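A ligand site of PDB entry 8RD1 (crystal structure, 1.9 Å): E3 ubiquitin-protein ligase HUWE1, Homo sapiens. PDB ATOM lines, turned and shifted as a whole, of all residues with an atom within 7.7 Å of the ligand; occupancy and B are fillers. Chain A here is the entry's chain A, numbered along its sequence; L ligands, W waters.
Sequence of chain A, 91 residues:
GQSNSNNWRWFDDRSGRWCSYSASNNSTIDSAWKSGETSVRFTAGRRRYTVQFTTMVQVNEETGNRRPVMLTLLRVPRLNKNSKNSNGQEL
Trp 10 touches the ligand. CD1 of Tyr 21 touches C6 of the ligand (3.6 Å). CE2 of Phe 42 touches C6 of the ligand, 3.9 Å away. Ala 44 touches the ligand. Tyr 49 touches the ligand. Hydrophobic or aromatic side chains within 4 Å of the ligand: Trp 10, Tyr 21, Phe 42, Ala 44 and Tyr 49. Within 4 Å of the ligand: Trp 10, Tyr 21, Ser 22, Asn 25, Phe 42, Ala 44, Tyr 49, Gln 58 and Arg 67. The nearest printed residue that does not touch the ligand is Arg 47 (4.9 Å).
An oxygen (O2) of the ligand is in hydrogen-bond range of the side-chain amide nitrogen (ND2) of Asn 25 (2.9 Å). The guanidinium group of Arg 67 is in salt-bridge range of an oxygen (O4) of the ligand, at 3.8 Å. NE2 of Gln 58 is in hydrogen-bond range of O1 of the ligand (2.9 Å). The backbone NH (N) of Ser 22 is in hydrogen-bond range of an oxygen (O2) of the ligand (3.0 Å).
Water W2 bridges OH of Tyr 49 (2.6 Å) and O5 of the ligand (2.7 Å).
The side-chain hydroxyl of Tyr 21 is in hydrogen-bond range of the side-chain amide oxygen of Gln 58 (2.7 Å). The backbone carbonyl oxygen (O) of Thr 43 sits at hydrogen-bond distance from the side-chain amide nitrogen (ND2) of Asn 25 (3.1 Å). The side-chain amide nitrogen of Asn 65 sits close to the guanidinium group of Arg 67. O of Arg 67 is in hydrogen-bond range of N of Gln 58, at 2.8 Å. O of Phe 42 sits at hydrogen-bond distance from N of Tyr 49 (2.9 Å). The side-chain hydroxyl (OG) of Ser 22 sits at hydrogen-bond distance from the backbone NH (N) of Asn 25 (3.2 Å). O of Trp 10 sits at hydrogen-bond distance from N of Cys 19 (2.8 Å). O of Ser 20 sits at hydrogen-bond distance from NE1 of Trp 10.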
ATOM      1  N   TRP A  10       1.273 -23.869 -24.106  1.00  0.00           N
ATOM      2  CA  TRP A  10       0.936 -25.211 -23.613  1.00  0.00           C
ATOM      3  C   TRP A  10       2.237 -25.891 -23.199  1.00  0.00           C
ATOM      4  O   TRP A  10       3.281 -25.649 -23.814  1.00  0.00           O
ATOM      5  CB  TRP A  10       0.170 -26.046 -24.666  1.00  0.00           C
ATOM      6  CG  TRP A  10       0.929 -26.257 -25.951  1.00  0.00           C
ATOM      7  CD1 TRP A  10       0.955 -25.413 -27.019  1.00  0.00           C
ATOM      8  CD2 TRP A  10       1.786 -27.356 -26.297  1.00  0.00           C
ATOM      9  NE1 TRP A  10       1.753 -25.931 -28.010  1.00  0.00           N
ATOM     10  CE2 TRP A  10       2.300 -27.111 -27.582  1.00  0.00           C
ATOM     11  CE3 TRP A  10       2.207 -28.519 -25.625  1.00  0.00           C
ATOM     12  CZ2 TRP A  10       3.236 -27.955 -28.195  1.00  0.00           C
ATOM     13  CZ3 TRP A  10       3.058 -29.384 -26.273  1.00  0.00           C
ATOM     14  CH2 TRP A  10       3.584 -29.086 -27.524  1.00  0.00           C
ATOM     15  N   PHE A  11       2.177 -26.723 -22.143  1.00  0.00           N
ATOM     16  CA  PHE A  11       3.383 -27.346 -21.627  1.00  0.00           C
ATOM     17  C   PHE A  11       3.675 -28.686 -22.306  1.00  0.00           C
ATOM     18  O   PHE A  11       2.820 -29.562 -22.329  1.00  0.00           O
ATOM     19  CB  PHE A  11       3.345 -27.504 -20.123  1.00  0.00           C
ATOM     20  CG  PHE A  11       4.676 -27.877 -19.519  1.00  0.00           C
ATOM     21  CD1 PHE A  11       5.672 -26.933 -19.382  1.00  0.00           C
ATOM     22  CD2 PHE A  11       4.927 -29.174 -19.092  1.00  0.00           C
ATOM     23  CE1 PHE A  11       6.884 -27.258 -18.781  1.00  0.00           C
ATOM     24  CE2 PHE A  11       6.158 -29.498 -18.503  1.00  0.00           C
ATOM     25  CZ  PHE A  11       7.116 -28.530 -18.342  1.00  0.00           C
ATOM     26  N   ASP A  12       4.902 -28.828 -22.808  1.00  0.00           N
ATOM     27  CA  ASP A  12       5.392 -30.043 -23.458  1.00  0.00           C
ATOM     28  C   ASP A  12       6.213 -30.800 -22.431  1.00  0.00           C
ATOM     29  O   ASP A  12       7.354 -30.401 -22.176  1.00  0.00           O
ATOM     30  CB  ASP A  12       6.259 -29.636 -24.663  1.00  0.00           C
ATOM     31  CG  ASP A  12       6.758 -30.775 -25.500  1.00  0.00           C
ATOM     32  OD1 ASP A  12       6.774 -31.917 -24.999  1.00  0.00           O
ATOM     33  OD2 ASP A  12       7.138 -30.526 -26.671  1.00  0.00           O
ATOM     34  N   ARG A  14       7.519 -33.704 -22.749  1.00  0.00           N
ATOM     35  CA  ARG A  14       8.586 -34.482 -23.399  1.00  0.00           C
ATOM     36  C   ARG A  14       9.878 -33.639 -23.321  1.00  0.00           C
ATOM     37  O   ARG A  14      10.906 -34.142 -22.902  1.00  0.00           O
ATOM     38  CB  ARG A  14       8.174 -34.797 -24.860  1.00  0.00           C
ATOM     39  CG  ARG A  14       9.159 -35.549 -25.781  1.00  0.00           C
ATOM     40  CD  ARG A  14       8.450 -35.848 -27.110  1.00  0.00           C
ATOM     41  NE  ARG A  14       9.251 -36.570 -28.104  1.00  0.00           N
ATOM     42  CZ  ARG A  14       9.363 -37.893 -28.222  1.00  0.00           C
ATOM     43  NH1 ARG A  14       8.755 -38.715 -27.354  1.00  0.00           N
ATOM     44  NH2 ARG A  14      10.116 -38.424 -29.191  1.00  0.00           N
ATOM     45  N   CYS A  19       5.450 -24.159 -24.709  1.00  0.00           N
ATOM     46  CA  CYS A  19       5.479 -23.997 -26.167  1.00  0.00           C
ATOM     47  C   CYS A  19       4.382 -23.095 -26.660  1.00  0.00           C
ATOM     48  O   CYS A  19       3.291 -23.081 -26.117  1.00  0.00           O
ATOM     49  CB  CYS A  19       5.370 -25.367 -26.827  1.00  0.00           C
ATOM     50  SG  CYS A  19       6.756 -26.473 -26.479  1.00  0.00           S
ATOM     51  N   SER A  20       4.638 -22.393 -27.766  1.00  0.00           N
ATOM     52  CA  SER A  20       3.666 -21.491 -28.364  1.00  0.00           C
ATOM     53  C   SER A  20       2.654 -22.217 -29.244  1.00  0.00           C
ATOM     54  O   SER A  20       2.934 -23.297 -29.782  1.00  0.00           O
ATOM     55  CB  SER A  20       4.365 -20.436 -29.222  1.00  0.00           C
ATOM     56  OG  SER A  20       5.142 -19.562 -28.427  1.00  0.00           O
ATOM     57  N   TYR A  21       1.476 -21.634 -29.373  1.00  0.00           N
ATOM     58  CA  TYR A  21       0.478 -22.107 -30.298  1.00  0.00           C
ATOM     59  C   TYR A  21       0.804 -21.481 -31.655  1.00  0.00           C
ATOM     60  O   TYR A  21       1.522 -20.480 -31.739  1.00  0.00           O
ATOM     61  CB  TYR A  21      -0.913 -21.624 -29.852  1.00  0.00           C
ATOM     62  CG  TYR A  21      -1.483 -22.475 -28.740  1.00  0.00           C
ATOM     63  CD1 TYR A  21      -2.059 -23.710 -29.009  1.00  0.00           C
ATOM     64  CD2 TYR A  21      -1.412 -22.058 -27.423  1.00  0.00           C
ATOM     65  CE1 TYR A  21      -2.533 -24.517 -27.987  1.00  0.00           C
ATOM     66  CE2 TYR A  21      -1.898 -22.852 -26.387  1.00  0.00           C
ATOM     67  CZ  TYR A  21      -2.460 -24.084 -26.675  1.00  0.00           C
ATOM     68  OH  TYR A  21      -2.963 -24.891 -25.699  1.00  0.00           O
ATOM     69  N   SER A  22       0.187 -22.018 -32.739  1.00  0.00           N
ATOM     70  CA  SER A  22       0.286 -21.368 -34.043  1.00  0.00           C
ATOM     71  C   SER A  22      -0.464 -20.025 -33.937  1.00  0.00           C
ATOM     72  O   SER A  22      -1.308 -19.872 -33.039  1.00  0.00           O
ATOM     73  CB  SER A  22      -0.354 -22.236 -35.114  1.00  0.00           C
ATOM     74  OG  SER A  22      -1.757 -22.330 -34.906  1.00  0.00           O
ATOM     75  N   ALA A  23      -0.165 -19.059 -34.818  1.00  0.00           N
ATOM     76  CA  ALA A  23      -0.822 -17.757 -34.766  1.00  0.00           C
ATOM     77  C   ALA A  23      -2.350 -17.883 -34.829  1.00  0.00           C
ATOM     78  O   ALA A  23      -3.039 -17.236 -34.035  1.00  0.00           O
ATOM     79  CB  ALA A  23      -0.332 -16.882 -35.905  1.00  0.00           C
ATOM     80  N   SER A  24      -2.870 -18.772 -35.678  1.00  0.00           N
ATOM     81  CA  SER A  24      -4.317 -18.947 -35.806  1.00  0.00           C
ATOM     82  C   SER A  24      -4.927 -19.602 -34.581  1.00  0.00           C
ATOM     83  O   SER A  24      -6.010 -19.190 -34.160  1.00  0.00           O
ATOM     84  CB  SER A  24      -4.679 -19.713 -37.066  1.00  0.00           C
ATOM     85  OG  SER A  24      -3.886 -20.868 -37.219  1.00  0.00           O
ATOM     86  N   ASN A  25      -4.254 -20.604 -33.973  1.00  0.00           N
ATOM     87  CA  ASN A  25      -4.807 -21.246 -32.765  1.00  0.00           C
ATOM     88  C   ASN A  25      -4.748 -20.279 -31.583  1.00  0.00           C
ATOM     89  O   ASN A  25      -5.701 -20.193 -30.806  1.00  0.00           O
ATOM     90  CB  ASN A  25      -4.099 -22.557 -32.453  1.00  0.00           C
ATOM     91  CG  ASN A  25      -4.508 -23.671 -33.385  1.00  0.00           C
ATOM     92  OD1 ASN A  25      -5.565 -23.619 -34.017  1.00  0.00           O
ATOM     93  ND2 ASN A  25      -3.708 -24.735 -33.470  1.00  0.00           N
ATOM     94  N   ASN A  26      -3.678 -19.474 -31.488  1.00  0.00           N
ATOM     95  CA  ASN A  26      -3.569 -18.472 -30.436  1.00  0.00           C
ATOM     96  C   ASN A  26      -4.715 -17.444 -30.563  1.00  0.00           C
ATOM     97  O   ASN A  26      -5.346 -17.084 -29.553  1.00  0.00           O
ATOM     98  CB  ASN A  26      -2.235 -17.756 -30.502  1.00  0.00           C
ATOM     99  CG  ASN A  26      -2.044 -16.862 -29.312  1.00  0.00           C
ATOM    100  OD1 ASN A  26      -1.717 -17.323 -28.220  1.00  0.00           O
ATOM    101  ND2 ASN A  26      -2.307 -15.583 -29.457  1.00  0.00           N
ATOM    102  N   ILE A  29      -8.031 -19.136 -29.484  1.00  0.00           N
ATOM    103  CA  ILE A  29      -8.104 -19.258 -28.029  1.00  0.00           C
ATOM    104  C   ILE A  29      -8.358 -17.891 -27.398  1.00  0.00           C
ATOM    105  O   ILE A  29      -9.260 -17.751 -26.574  1.00  0.00           O
ATOM    106  CB  ILE A  29      -6.832 -19.938 -27.442  1.00  0.00           C
ATOM    107  CG1 ILE A  29      -6.728 -21.423 -27.908  1.00  0.00           C
ATOM    108  CG2 ILE A  29      -6.825 -19.854 -25.919  1.00  0.00           C
ATOM    109  CD1 ILE A  29      -5.290 -21.972 -27.888  1.00  0.00           C
ATOM    110  N   PHE A  42     -10.284 -26.209 -30.935  1.00  0.00           N
ATOM    111  CA  PHE A  42      -9.415 -25.858 -32.054  1.00  0.00           C
ATOM    112  C   PHE A  42      -8.734 -27.132 -32.585  1.00  0.00           C
ATOM    113  O   PHE A  42      -8.788 -28.200 -31.962  1.00  0.00           O
ATOM    114  CB  PHE A  42      -8.405 -24.753 -31.676  1.00  0.00           C
ATOM    115  CG  PHE A  42      -7.310 -25.202 -30.742  1.00  0.00           C
ATOM    116  CD1 PHE A  42      -7.473 -25.149 -29.360  1.00  0.00           C
ATOM    117  CD2 PHE A  42      -6.136 -25.733 -31.230  1.00  0.00           C
ATOM    118  CE1 PHE A  42      -6.480 -25.608 -28.521  1.00  0.00           C
ATOM    119  CE2 PHE A  42      -5.149 -26.167 -30.375  1.00  0.00           C
ATOM    120  CZ  PHE A  42      -5.361 -26.176 -29.045  1.00  0.00           C
ATOM    121  N   THR A  43      -8.125 -27.044 -33.764  1.00  0.00           N
ATOM    122  CA  THR A  43      -7.444 -28.172 -34.387  1.00  0.00           C
ATOM    123  C   THR A  43      -5.997 -27.809 -34.693  1.00  0.00           C
ATOM    124  O   THR A  43      -5.677 -26.636 -34.862  1.00  0.00           O
ATOM    125  CB  THR A  43      -8.204 -28.573 -35.672  1.00  0.00           C
ATOM    126  OG1 THR A  43      -7.978 -27.580 -36.675  1.00  0.00           O
ATOM    127  CG2 THR A  43      -9.725 -28.717 -35.466  1.00  0.00           C
ATOM    128  N   ALA A  44      -5.131 -28.799 -34.756  1.00  0.00           N
ATOM    129  CA  ALA A  44      -3.757 -28.643 -35.237  1.00  0.00           C
ATOM    130  C   ALA A  44      -3.511 -29.862 -36.096  1.00  0.00           C
ATOM    131  O   ALA A  44      -3.363 -30.958 -35.565  1.00  0.00           O
ATOM    132  CB  ALA A  44      -2.766 -28.543 -34.098  1.00  0.00           C
ATOM    133  N   GLY A  45      -3.681 -29.724 -37.401  1.00  0.00           N
ATOM    134  CA  GLY A  45      -3.584 -30.834 -38.329  1.00  0.00           C
ATOM    135  C   GLY A  45      -4.721 -31.816 -38.086  1.00  0.00           C
ATOM    136  O   GLY A  45      -5.880 -31.407 -38.019  1.00  0.00           O
ATOM    137  N   ARG A  47      -5.085 -33.318 -35.155  1.00  0.00           N
ATOM    138  CA  ARG A  47      -5.367 -33.299 -33.727  1.00  0.00           C
ATOM    139  C   ARG A  47      -6.543 -32.345 -33.383  1.00  0.00           C
ATOM    140  O   ARG A  47      -6.696 -31.286 -34.007  1.00  0.00           O
ATOM    141  CB  ARG A  47      -4.096 -32.899 -32.947  1.00  0.00           C
ATOM    142  CG  ARG A  47      -2.818 -33.713 -33.246  1.00  0.00           C
ATOM    143  CD  ARG A  47      -2.785 -35.082 -32.563  1.00  0.00           C
ATOM    144  NE  ARG A  47      -3.761 -36.041 -33.094  1.00  0.00           N
ATOM    145  CZ  ARG A  47      -3.595 -36.777 -34.196  1.00  0.00           C
ATOM    146  NH1 ARG A  47      -2.504 -36.641 -34.947  1.00  0.00           N
ATOM    147  NH2 ARG A  47      -4.535 -37.637 -34.571  1.00  0.00           N
ATOM    148  N   TYR A  49      -8.545 -30.451 -30.071  1.00  0.00           N
ATOM    149  CA  TYR A  49      -8.365 -30.098 -28.675  1.00  0.00           C
ATOM    150  C   TYR A  49      -9.446 -29.207 -28.165  1.00  0.00           C
ATOM    151  O   TYR A  49     -10.059 -28.467 -28.946  1.00  0.00           O
ATOM    152  CB  TYR A  49      -7.069 -29.311 -28.473  1.00  0.00           C
ATOM    153  CG  TYR A  49      -5.826 -29.960 -29.053  1.00  0.00           C
ATOM    154  CD1 TYR A  49      -5.354 -29.601 -30.304  1.00  0.00           C
ATOM    155  CD2 TYR A  49      -5.123 -30.916 -28.337  1.00  0.00           C
ATOM    156  CE1 TYR A  49      -4.166 -30.083 -30.787  1.00  0.00           C
ATOM    157  CE2 TYR A  49      -3.975 -31.492 -28.857  1.00  0.00           C
ATOM    158  CZ  TYR A  49      -3.472 -31.043 -30.068  1.00  0.00           C
ATOM    159  OH  TYR A  49      -2.320 -31.509 -30.625  1.00  0.00           O
ATOM    160  N   GLN A  58      -5.506 -27.982 -21.596  1.00  0.00           N
ATOM    161  CA  GLN A  58      -5.818 -28.393 -22.951  1.00  0.00           C
ATOM    162  C   GLN A  58      -6.043 -29.905 -22.900  1.00  0.00           C
ATOM    163  O   GLN A  58      -5.192 -30.645 -22.386  1.00  0.00           O
ATOM    164  CB  GLN A  58      -4.669 -28.075 -23.903  1.00  0.00           C
ATOM    165  CG  GLN A  58      -4.894 -28.560 -25.338  1.00  0.00           C
ATOM    166  CD  GLN A  58      -3.611 -28.415 -26.128  1.00  0.00           C
ATOM    167  OE1 GLN A  58      -3.310 -27.348 -26.662  1.00  0.00           O
ATOM    168  NE2 GLN A  58      -2.816 -29.475 -26.222  1.00  0.00           N
ATOM    169  N   ASN A  60      -6.863 -33.292 -25.188  1.00  0.00           N
ATOM    170  CA  ASN A  60      -6.876 -33.909 -26.515  1.00  0.00           C
ATOM    171  C   ASN A  60      -8.229 -34.658 -26.571  1.00  0.00           C
ATOM    172  O   ASN A  60      -8.505 -35.514 -25.739  1.00  0.00           O
ATOM    173  CB  ASN A  60      -5.701 -34.853 -26.635  1.00  0.00           C
ATOM    174  CG  ASN A  60      -5.611 -35.558 -27.957  1.00  0.00           C
ATOM    175  OD1 ASN A  60      -6.614 -36.097 -28.488  1.00  0.00           O
ATOM    176  ND2 ASN A  60      -4.409 -35.583 -28.500  1.00  0.00           N
ATOM    177  N   ASN A  65      -5.611 -36.870 -23.262  1.00  0.00           N
ATOM    178  CA  ASN A  65      -4.374 -36.350 -22.695  1.00  0.00           C
ATOM    179  C   ASN A  65      -4.527 -34.874 -22.306  1.00  0.00           C
ATOM    180  O   ASN A  65      -5.063 -34.076 -23.093  1.00  0.00           O
ATOM    181  CB  ASN A  65      -3.205 -36.489 -23.650  1.00  0.00           C
ATOM    182  CG  ASN A  65      -1.895 -36.086 -23.009  1.00  0.00           C
ATOM    183  OD1 ASN A  65      -1.515 -36.579 -21.942  1.00  0.00           O
ATOM    184  ND2 ASN A  65      -1.166 -35.176 -23.637  1.00  0.00           N
ATOM    185  N   ARG A  67      -2.740 -31.375 -21.089  1.00  0.00           N
ATOM    186  CA  ARG A  67      -1.530 -30.578 -21.099  1.00  0.00           C
ATOM    187  C   ARG A  67      -1.908 -29.248 -20.474  1.00  0.00           C
ATOM    188  O   ARG A  67      -2.889 -28.627 -20.927  1.00  0.00           O
ATOM    189  CB  ARG A  67      -1.008 -30.330 -22.516  1.00  0.00           C
ATOM    190  CG  ARG A  67      -0.485 -31.590 -23.197  1.00  0.00           C
ATOM    191  CD  ARG A  67       0.024 -31.326 -24.623  1.00  0.00           C
ATOM    192  NE  ARG A  67       1.313 -31.989 -24.890  1.00  0.00           N
ATOM    193  CZ  ARG A  67       1.503 -33.205 -25.402  1.00  0.00           C
ATOM    194  NH1 ARG A  67       2.724 -33.655 -25.607  1.00  0.00           N
ATOM    195  NH2 ARG A  67       0.482 -33.982 -25.670  1.00  0.00           N
HETATM  196  C1  LIG L   1       0.745 -27.714 -31.486  1.00  0.00           C
HETATM  197  C2  LIG L   1       0.036 -30.021 -28.748  1.00  0.00           C
HETATM  198  C3  LIG L   1      -1.261 -27.886 -29.554  1.00  0.00           C
HETATM  199  C4  LIG L   1      -0.352 -25.715 -32.552  1.00  0.00           C
HETATM  200  C5  LIG L   1       0.719 -28.772 -30.592  1.00  0.00           C
HETATM  201  C6  LIG L   1      -1.302 -26.887 -30.512  1.00  0.00           C
HETATM  202  C7  LIG L   1       1.862 -31.759 -28.694  1.00  0.00           C
HETATM  203  C8  LIG L   1       2.051 -32.966 -29.627  1.00  0.00           C
HETATM  204  C9  LIG L   1      -0.253 -28.855 -29.619  1.00  0.00           C
HETATM  205  C10 LIG L   1       1.637 -29.927 -30.425  1.00  0.00           C
HETATM  206  C11 LIG L   1      -0.300 -26.795 -31.487  1.00  0.00           C
HETATM  207  N1  LIG L   1       1.160 -30.626 -29.307  1.00  0.00           N
HETATM  208  O1  LIG L   1      -0.507 -30.375 -27.734  1.00  0.00           O
HETATM  209  O2  LIG L   1      -1.084 -24.722 -32.353  1.00  0.00           O
HETATM  210  O3  LIG L   1       0.366 -25.858 -33.584  1.00  0.00           O
HETATM  211  O4  LIG L   1       3.053 -33.687 -29.368  1.00  0.00           O
HETATM  212  O5  LIG L   1       1.214 -33.197 -30.531  1.00  0.00           O
HETATM  213  O6  LIG L   1       2.641 -30.207 -31.038  1.00  0.00           O
HETATM  214  O   HOH W   1       3.094 -23.727 -33.962  1.00  0.00           O
HETATM  215  O   HOH W   2      -1.259 -33.680 -29.624  1.00  0.00           O
